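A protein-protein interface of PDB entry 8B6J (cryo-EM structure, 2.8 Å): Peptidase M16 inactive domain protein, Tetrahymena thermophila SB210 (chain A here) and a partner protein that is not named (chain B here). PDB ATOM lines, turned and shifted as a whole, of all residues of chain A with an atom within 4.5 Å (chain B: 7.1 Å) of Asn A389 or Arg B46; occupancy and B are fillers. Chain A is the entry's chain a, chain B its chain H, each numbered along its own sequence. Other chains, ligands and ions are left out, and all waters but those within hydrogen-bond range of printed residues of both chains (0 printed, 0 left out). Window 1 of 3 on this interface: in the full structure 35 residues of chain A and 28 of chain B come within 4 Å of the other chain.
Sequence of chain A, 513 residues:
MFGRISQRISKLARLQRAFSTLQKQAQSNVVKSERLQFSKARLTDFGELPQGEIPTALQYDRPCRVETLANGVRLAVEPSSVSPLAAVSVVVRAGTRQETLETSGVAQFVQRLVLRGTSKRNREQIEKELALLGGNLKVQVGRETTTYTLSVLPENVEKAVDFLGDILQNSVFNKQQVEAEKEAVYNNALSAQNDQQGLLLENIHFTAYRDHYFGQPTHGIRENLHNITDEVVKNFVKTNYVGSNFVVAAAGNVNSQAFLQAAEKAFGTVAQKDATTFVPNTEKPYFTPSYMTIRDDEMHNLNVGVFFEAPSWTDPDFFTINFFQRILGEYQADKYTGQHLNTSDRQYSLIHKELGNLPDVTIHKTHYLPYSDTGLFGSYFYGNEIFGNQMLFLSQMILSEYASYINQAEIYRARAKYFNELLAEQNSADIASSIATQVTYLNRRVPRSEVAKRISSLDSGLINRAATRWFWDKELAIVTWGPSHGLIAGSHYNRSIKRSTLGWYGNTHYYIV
Printed residues of chain B that touch a printed residue of chain A: Ser B44 and Arg B46. Among the printed residues, 5 pairs touch across the chains. Among the printed residues, no Asp or Glu carboxylate lies within 4 Å of a Lys or Arg side-chain nitrogen of the other chain.
O of Ile A512 touches NH2 of Arg B46, at 3.6 Å. Val A513 touches Ser B44. Val A513 touches Arg B46.
Asn A389 touches just one residue of chain B: Arg B46. Of chain A, only Asn A389 (2.9 Å), His A509 (3.0 Å), Ile A512 (3.6 Å) and Val A513 (3.2 Å) come within 4 Å of Arg B46. Printed residues of chain A within 4 Å of Ser B44: Val A513 (2.8 Å). Of the printed residues of chain B, His A509 touches Arg B46 (3.0 Å). Of the printed residues of chain B, Ile A512 touches Arg B46. Printed residues of chain B within 4 Å of Val A513: Ser B44 (2.8 Å) and Arg B46 (3.2 Å). The nearest printed residue of chain B that does not touch Asn A389 is Ser B44 (8.7 Å).
The side-chain amide nitrogen (ND2) of Asn A389 lies close to the guanidinium group (NH1) of Arg B46 (2.9 Å). The guanidinium group of Arg B46 is in hydrogen-bond range of the backbone carbonyl oxygen of His A509, 3.0 Å away.
The chain-end carboxylate of Val A513 lies within hydrogen-bond range of the side-chain amide nitrogen of Gln A390 (3.1 Å). The backbone NH (N) of Arg B46 sits at hydrogen-bond distance from the side-chain hydroxyl (OG) of Ser B44, at 2.8 Å. The backbone carbonyl oxygen (O) of Ile A512 lies within hydrogen-bond range of the side-chain amide nitrogen (NE2) of Gln A390 (2.6 Å).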
ATOM      1  N   PHE A 387      19.231 -26.221 -29.349  1.00  0.00           N
ATOM      2  CA  PHE A 387      19.195 -26.272 -27.895  1.00  0.00           C
ATOM      3  C   PHE A 387      19.798 -27.561 -27.349  1.00  0.00           C
ATOM      4  O   PHE A 387      19.485 -27.954 -26.221  1.00  0.00           O
ATOM      5  CB  PHE A 387      17.759 -26.110 -27.397  1.00  0.00           C
ATOM      6  CG  PHE A 387      17.173 -24.760 -27.678  1.00  0.00           C
ATOM      7  CD1 PHE A 387      17.523 -23.666 -26.908  1.00  0.00           C
ATOM      8  CD2 PHE A 387      16.271 -24.582 -28.712  1.00  0.00           C
ATOM      9  CE1 PHE A 387      16.989 -22.422 -27.164  1.00  0.00           C
ATOM     10  CE2 PHE A 387      15.735 -23.339 -28.973  1.00  0.00           C
ATOM     11  CZ  PHE A 387      16.093 -22.259 -28.198  1.00  0.00           C
ATOM     12  N   GLY A 388      20.658 -28.219 -28.124  1.00  0.00           N
ATOM     13  CA  GLY A 388      21.268 -29.465 -27.702  1.00  0.00           C
ATOM     14  C   GLY A 388      21.801 -29.419 -26.286  1.00  0.00           C
ATOM     15  O   GLY A 388      21.311 -30.139 -25.411  1.00  0.00           O
ATOM     16  N   ASN A 389      22.791 -28.558 -26.041  1.00  0.00           N
ATOM     17  CA  ASN A 389      23.364 -28.463 -24.703  1.00  0.00           C
ATOM     18  C   ASN A 389      22.285 -28.188 -23.667  1.00  0.00           C
ATOM     19  O   ASN A 389      22.326 -28.733 -22.557  1.00  0.00           O
ATOM     20  CB  ASN A 389      24.429 -27.369 -24.661  1.00  0.00           C
ATOM     21  CG  ASN A 389      25.536 -27.596 -25.665  1.00  0.00           C
ATOM     22  OD1 ASN A 389      25.283 -27.935 -26.819  1.00  0.00           O
ATOM     23  ND2 ASN A 389      26.776 -27.422 -25.226  1.00  0.00           N
ATOM     24  N   GLN A 390      21.299 -27.362 -24.015  1.00  0.00           N
ATOM     25  CA  GLN A 390      20.242 -27.047 -23.061  1.00  0.00           C
ATOM     26  C   GLN A 390      19.493 -28.306 -22.651  1.00  0.00           C
ATOM     27  O   GLN A 390      19.168 -28.488 -21.472  1.00  0.00           O
ATOM     28  CB  GLN A 390      19.285 -26.015 -23.653  1.00  0.00           C
ATOM     29  CG  GLN A 390      19.809 -24.592 -23.603  1.00  0.00           C
ATOM     30  CD  GLN A 390      21.124 -24.427 -24.334  1.00  0.00           C
ATOM     31  OE1 GLN A 390      21.216 -24.678 -25.535  1.00  0.00           O
ATOM     32  NE2 GLN A 390      22.155 -24.010 -23.609  1.00  0.00           N
ATOM     33  N   MET A 391      19.214 -29.192 -23.606  1.00  0.00           N
ATOM     34  CA  MET A 391      18.600 -30.467 -23.264  1.00  0.00           C
ATOM     35  C   MET A 391      19.594 -31.423 -22.619  1.00  0.00           C
ATOM     36  O   MET A 391      19.182 -32.320 -21.877  1.00  0.00           O
ATOM     37  CB  MET A 391      18.002 -31.114 -24.511  1.00  0.00           C
ATOM     38  CG  MET A 391      17.005 -30.244 -25.250  1.00  0.00           C
ATOM     39  SD  MET A 391      16.327 -31.049 -26.713  1.00  0.00           S
ATOM     40  CE  MET A 391      17.797 -31.228 -27.716  1.00  0.00           C
ATOM     41  N   LEU A 392      20.889 -31.252 -22.888  1.00  0.00           N
ATOM     42  CA  LEU A 392      21.887 -32.188 -22.382  1.00  0.00           C
ATOM     43  C   LEU A 392      22.150 -31.991 -20.892  1.00  0.00           C
ATOM     44  O   LEU A 392      22.264 -32.970 -20.147  1.00  0.00           O
ATOM     45  CB  LEU A 392      23.183 -32.034 -23.177  1.00  0.00           C
ATOM     46  CG  LEU A 392      24.253 -33.105 -22.973  1.00  0.00           C
ATOM     47  CD1 LEU A 392      23.774 -34.452 -23.480  1.00  0.00           C
ATOM     48  CD2 LEU A 392      25.539 -32.700 -23.668  1.00  0.00           C
ATOM     49  N   PHE A 393      22.250 -30.743 -20.440  1.00  0.00           N
ATOM     50  CA  PHE A 393      22.627 -30.437 -19.067  1.00  0.00           C
ATOM     51  C   PHE A 393      21.444 -30.074 -18.178  1.00  0.00           C
ATOM     52  O   PHE A 393      21.649 -29.774 -16.999  1.00  0.00           O
ATOM     53  CB  PHE A 393      23.639 -29.287 -19.044  1.00  0.00           C
ATOM     54  CG  PHE A 393      24.960 -29.627 -19.670  1.00  0.00           C
ATOM     55  CD1 PHE A 393      25.958 -30.227 -18.927  1.00  0.00           C
ATOM     56  CD2 PHE A 393      25.207 -29.332 -20.998  1.00  0.00           C
ATOM     57  CE1 PHE A 393      27.175 -30.536 -19.498  1.00  0.00           C
ATOM     58  CE2 PHE A 393      26.423 -29.639 -21.575  1.00  0.00           C
ATOM     59  CZ  PHE A 393      27.407 -30.241 -20.823  1.00  0.00           C
ATOM     60  N   LEU A 487      27.330 -30.677 -30.921  1.00  0.00           N
ATOM     61  CA  LEU A 487      27.724 -31.464 -29.758  1.00  0.00           C
ATOM     62  C   LEU A 487      28.980 -32.302 -29.974  1.00  0.00           C
ATOM     63  O   LEU A 487      29.442 -32.940 -29.024  1.00  0.00           O
ATOM     64  CB  LEU A 487      26.571 -32.384 -29.344  1.00  0.00           C
ATOM     65  CG  LEU A 487      25.281 -31.686 -28.908  1.00  0.00           C
ATOM     66  CD1 LEU A 487      24.162 -32.695 -28.730  1.00  0.00           C
ATOM     67  CD2 LEU A 487      25.501 -30.905 -27.624  1.00  0.00           C
ATOM     68  N   HIS A 509      27.161 -24.541 -18.637  1.00  0.00           N
ATOM     69  CA  HIS A 509      26.895 -24.831 -20.039  1.00  0.00           C
ATOM     70  C   HIS A 509      25.414 -24.746 -20.380  1.00  0.00           C
ATOM     71  O   HIS A 509      25.068 -24.367 -21.503  1.00  0.00           O
ATOM     72  CB  HIS A 509      27.440 -26.213 -20.395  1.00  0.00           C
ATOM     73  CG  HIS A 509      28.934 -26.277 -20.410  1.00  0.00           C
ATOM     74  ND1 HIS A 509      29.671 -26.160 -21.568  1.00  0.00           N
ATOM     75  CD2 HIS A 509      29.829 -26.428 -19.406  1.00  0.00           C
ATOM     76  CE1 HIS A 509      30.956 -26.246 -21.278  1.00  0.00           C
ATOM     77  NE2 HIS A 509      31.080 -26.408 -19.973  1.00  0.00           N
ATOM     78  N   ILE A 512      24.288 -20.908 -21.001  1.00  0.00           N
ATOM     79  CA  ILE A 512      24.826 -20.324 -22.223  1.00  0.00           C
ATOM     80  C   ILE A 512      24.035 -20.864 -23.406  1.00  0.00           C
ATOM     81  O   ILE A 512      23.954 -22.081 -23.613  1.00  0.00           O
ATOM     82  CB  ILE A 512      26.322 -20.622 -22.351  1.00  0.00           C
ATOM     83  CG1 ILE A 512      27.081 -19.993 -21.180  1.00  0.00           C
ATOM     84  CG2 ILE A 512      26.849 -20.103 -23.679  1.00  0.00           C
ATOM     85  CD1 ILE A 512      28.525 -20.420 -21.082  1.00  0.00           C
ATOM     86  N   VAL A 513      23.445 -19.958 -24.181  1.00  0.00           N
ATOM     87  CA  VAL A 513      22.560 -20.310 -25.290  1.00  0.00           C
ATOM     88  C   VAL A 513      21.239 -20.842 -24.749  1.00  0.00           C
ATOM     89  O   VAL A 513      20.279 -21.034 -25.495  1.00  0.00           O
ATOM     90  CB  VAL A 513      23.212 -21.331 -26.235  1.00  0.00           C
ATOM     91  CG1 VAL A 513      22.354 -21.533 -27.478  1.00  0.00           C
ATOM     92  CG2 VAL A 513      24.605 -20.873 -26.610  1.00  0.00           C
ATOM     93  OXT VAL A 513      21.096 -21.088 -23.553  1.00  0.00           O
ATOM     94  N   VAL B  41      26.272 -14.802 -35.041  1.00  0.00           N
ATOM     95  CA  VAL B  41      27.132 -14.806 -33.863  1.00  0.00           C
ATOM     96  C   VAL B  41      26.471 -14.055 -32.720  1.00  0.00           C
ATOM     97  O   VAL B  41      26.681 -14.382 -31.546  1.00  0.00           O
ATOM     98  CB  VAL B  41      28.512 -14.214 -34.221  1.00  0.00           C
ATOM     99  CG1 VAL B  41      29.011 -13.268 -33.136  1.00  0.00           C
ATOM    100  CG2 VAL B  41      29.517 -15.328 -34.454  1.00  0.00           C
ATOM    101  N   SER B  43      23.436 -14.171 -31.877  1.00  0.00           N
ATOM    102  CA  SER B  43      22.512 -15.065 -31.187  1.00  0.00           C
ATOM    103  C   SER B  43      23.215 -15.823 -30.069  1.00  0.00           C
ATOM    104  O   SER B  43      22.712 -15.899 -28.943  1.00  0.00           O
ATOM    105  CB  SER B  43      21.887 -16.039 -32.186  1.00  0.00           C
ATOM    106  OG  SER B  43      21.133 -15.349 -33.165  1.00  0.00           O
ATOM    107  N   SER B  44      24.386 -16.386 -30.360  1.00  0.00           N
ATOM    108  CA  SER B  44      25.113 -17.184 -29.385  1.00  0.00           C
ATOM    109  C   SER B  44      26.601 -17.147 -29.696  1.00  0.00           C
ATOM    110  O   SER B  44      27.006 -17.008 -30.853  1.00  0.00           O
ATOM    111  CB  SER B  44      24.626 -18.635 -29.376  1.00  0.00           C
ATOM    112  OG  SER B  44      25.633 -19.498 -28.881  1.00  0.00           O
ATOM    113  N   VAL B  45      27.412 -17.279 -28.644  1.00  0.00           N
ATOM    114  CA  VAL B  45      28.856 -17.368 -28.822  1.00  0.00           C
ATOM    115  C   VAL B  45      29.266 -18.718 -29.389  1.00  0.00           C
ATOM    116  O   VAL B  45      30.323 -18.827 -30.023  1.00  0.00           O
ATOM    117  CB  VAL B  45      29.586 -17.101 -27.492  1.00  0.00           C
ATOM    118  CG1 VAL B  45      29.373 -15.665 -27.051  1.00  0.00           C
ATOM    119  CG2 VAL B  45      29.113 -18.064 -26.413  1.00  0.00           C
ATOM    120  N   ARG B  46      28.451 -19.756 -29.189  1.00  0.00           N
ATOM    121  CA  ARG B  46      28.795 -21.081 -29.689  1.00  0.00           C
ATOM    122  C   ARG B  46      28.967 -21.097 -31.199  1.00  0.00           C
ATOM    123  O   ARG B  46      29.621 -22.002 -31.726  1.00  0.00           O
ATOM    124  CB  ARG B  46      27.722 -22.090 -29.281  1.00  0.00           C
ATOM    125  CG  ARG B  46      27.579 -22.258 -27.783  1.00  0.00           C
ATOM    126  CD  ARG B  46      26.640 -23.396 -27.434  1.00  0.00           C
ATOM    127  NE  ARG B  46      26.424 -23.490 -25.996  1.00  0.00           N
ATOM    128  CZ  ARG B  46      27.182 -24.190 -25.163  1.00  0.00           C
ATOM    129  NH1 ARG B  46      28.215 -24.895 -25.593  1.00  0.00           N
ATOM    130  NH2 ARG B  46      26.896 -24.182 -23.865  1.00  0.00           N
ATOM    131  N   TYR B  47      28.394 -20.123 -31.907  1.00  0.00           N
ATOM    132  CA  TYR B  47      28.557 -20.059 -33.352  1.00  0.00           C
ATOM    133  C   TYR B  47      29.988 -19.757 -33.772  1.00  0.00           C
ATOM    134  O   TYR B  47      30.314 -19.927 -34.951  1.00  0.00           O
ATOM    135  CB  TYR B  47      27.614 -19.010 -33.938  1.00  0.00           C
ATOM    136  CG  TYR B  47      26.193 -19.497 -34.093  1.00  0.00           C
ATOM    137  CD1 TYR B  47      25.819 -20.257 -35.190  1.00  0.00           C
ATOM    138  CD2 TYR B  47      25.229 -19.198 -33.144  1.00  0.00           C
ATOM    139  CE1 TYR B  47      24.525 -20.705 -35.338  1.00  0.00           C
ATOM    140  CE2 TYR B  47      23.931 -19.642 -33.284  1.00  0.00           C
ATOM    141  CZ  TYR B  47      23.586 -20.395 -34.382  1.00  0.00           C
ATOM    142  OH  TYR B  47      22.293 -20.840 -34.525  1.00  0.00           O
ATOM    143  N   TYR B  48      30.845 -19.311 -32.851  1.00  0.00           N
ATOM    144  CA  TYR B  48      32.240 -19.083 -33.202  1.00  0.00           C
ATOM    145  C   TYR B  48      32.978 -20.380 -33.506  1.00  0.00           C
ATOM    146  O   TYR B  48      34.007 -20.347 -34.188  1.00  0.00           O
ATOM    147  CB  TYR B  48      32.947 -18.324 -32.080  1.00  0.00           C
ATOM    148  CG  TYR B  48      32.678 -16.840 -32.116  1.00  0.00           C
ATOM    149  CD1 TYR B  48      33.323 -16.025 -33.034  1.00  0.00           C
ATOM    150  CD2 TYR B  48      31.776 -16.253 -31.241  1.00  0.00           C
ATOM    151  CE1 TYR B  48      33.081 -14.671 -33.079  1.00  0.00           C
ATOM    152  CE2 TYR B  48      31.528 -14.897 -31.278  1.00  0.00           C
ATOM    153  CZ  TYR B  48      32.183 -14.113 -32.200  1.00  0.00           C
ATOM    154  OH  TYR B  48      31.945 -12.760 -32.246  1.00  0.00           O
ATOM    155  N   HIS B  49      32.481 -21.515 -33.019  1.00  0.00           N
ATOM    156  CA  HIS B  49      33.023 -22.824 -33.378  1.00  0.00           C
ATOM    157  C   HIS B  49      32.375 -23.232 -34.694  1.00  0.00           C
ATOM    158  O   HIS B  49      31.410 -23.997 -34.730  1.00  0.00           O
ATOM    159  CB  HIS B  49      32.758 -23.840 -32.273  1.00  0.00           C
ATOM    160  CG  HIS B  49      33.354 -25.188 -32.534  1.00  0.00           C
ATOM    161  ND1 HIS B  49      34.691 -25.369 -32.815  1.00  0.00           N
ATOM    162  CD2 HIS B  49      32.796 -26.422 -32.549  1.00  0.00           C
ATOM    163  CE1 HIS B  49      34.930 -26.655 -32.995  1.00  0.00           C
ATOM    164  NE2 HIS B  49      33.797 -27.316 -32.839  1.00  0.00           N
ATOM    165  N   ASP B  50      32.919 -22.713 -35.790  1.00  0.00           N
ATOM    166  CA  ASP B  50      32.305 -22.805 -37.111  1.00  0.00           C
ATOM    167  C   ASP B  50      33.080 -23.737 -38.038  1.00  0.00           C
ATOM    168  O   ASP B  50      33.236 -23.464 -39.230  1.00  0.00           O
ATOM    169  CB  ASP B  50      32.186 -21.418 -37.735  1.00  0.00           C
ATOM    170  CG  ASP B  50      33.525 -20.722 -37.863  1.00  0.00           C
ATOM    171  OD1 ASP B  50      34.321 -21.120 -38.736  1.00  0.00           O
ATOM    172  OD2 ASP B  50      33.786 -19.779 -37.088  1.00  0.00           O
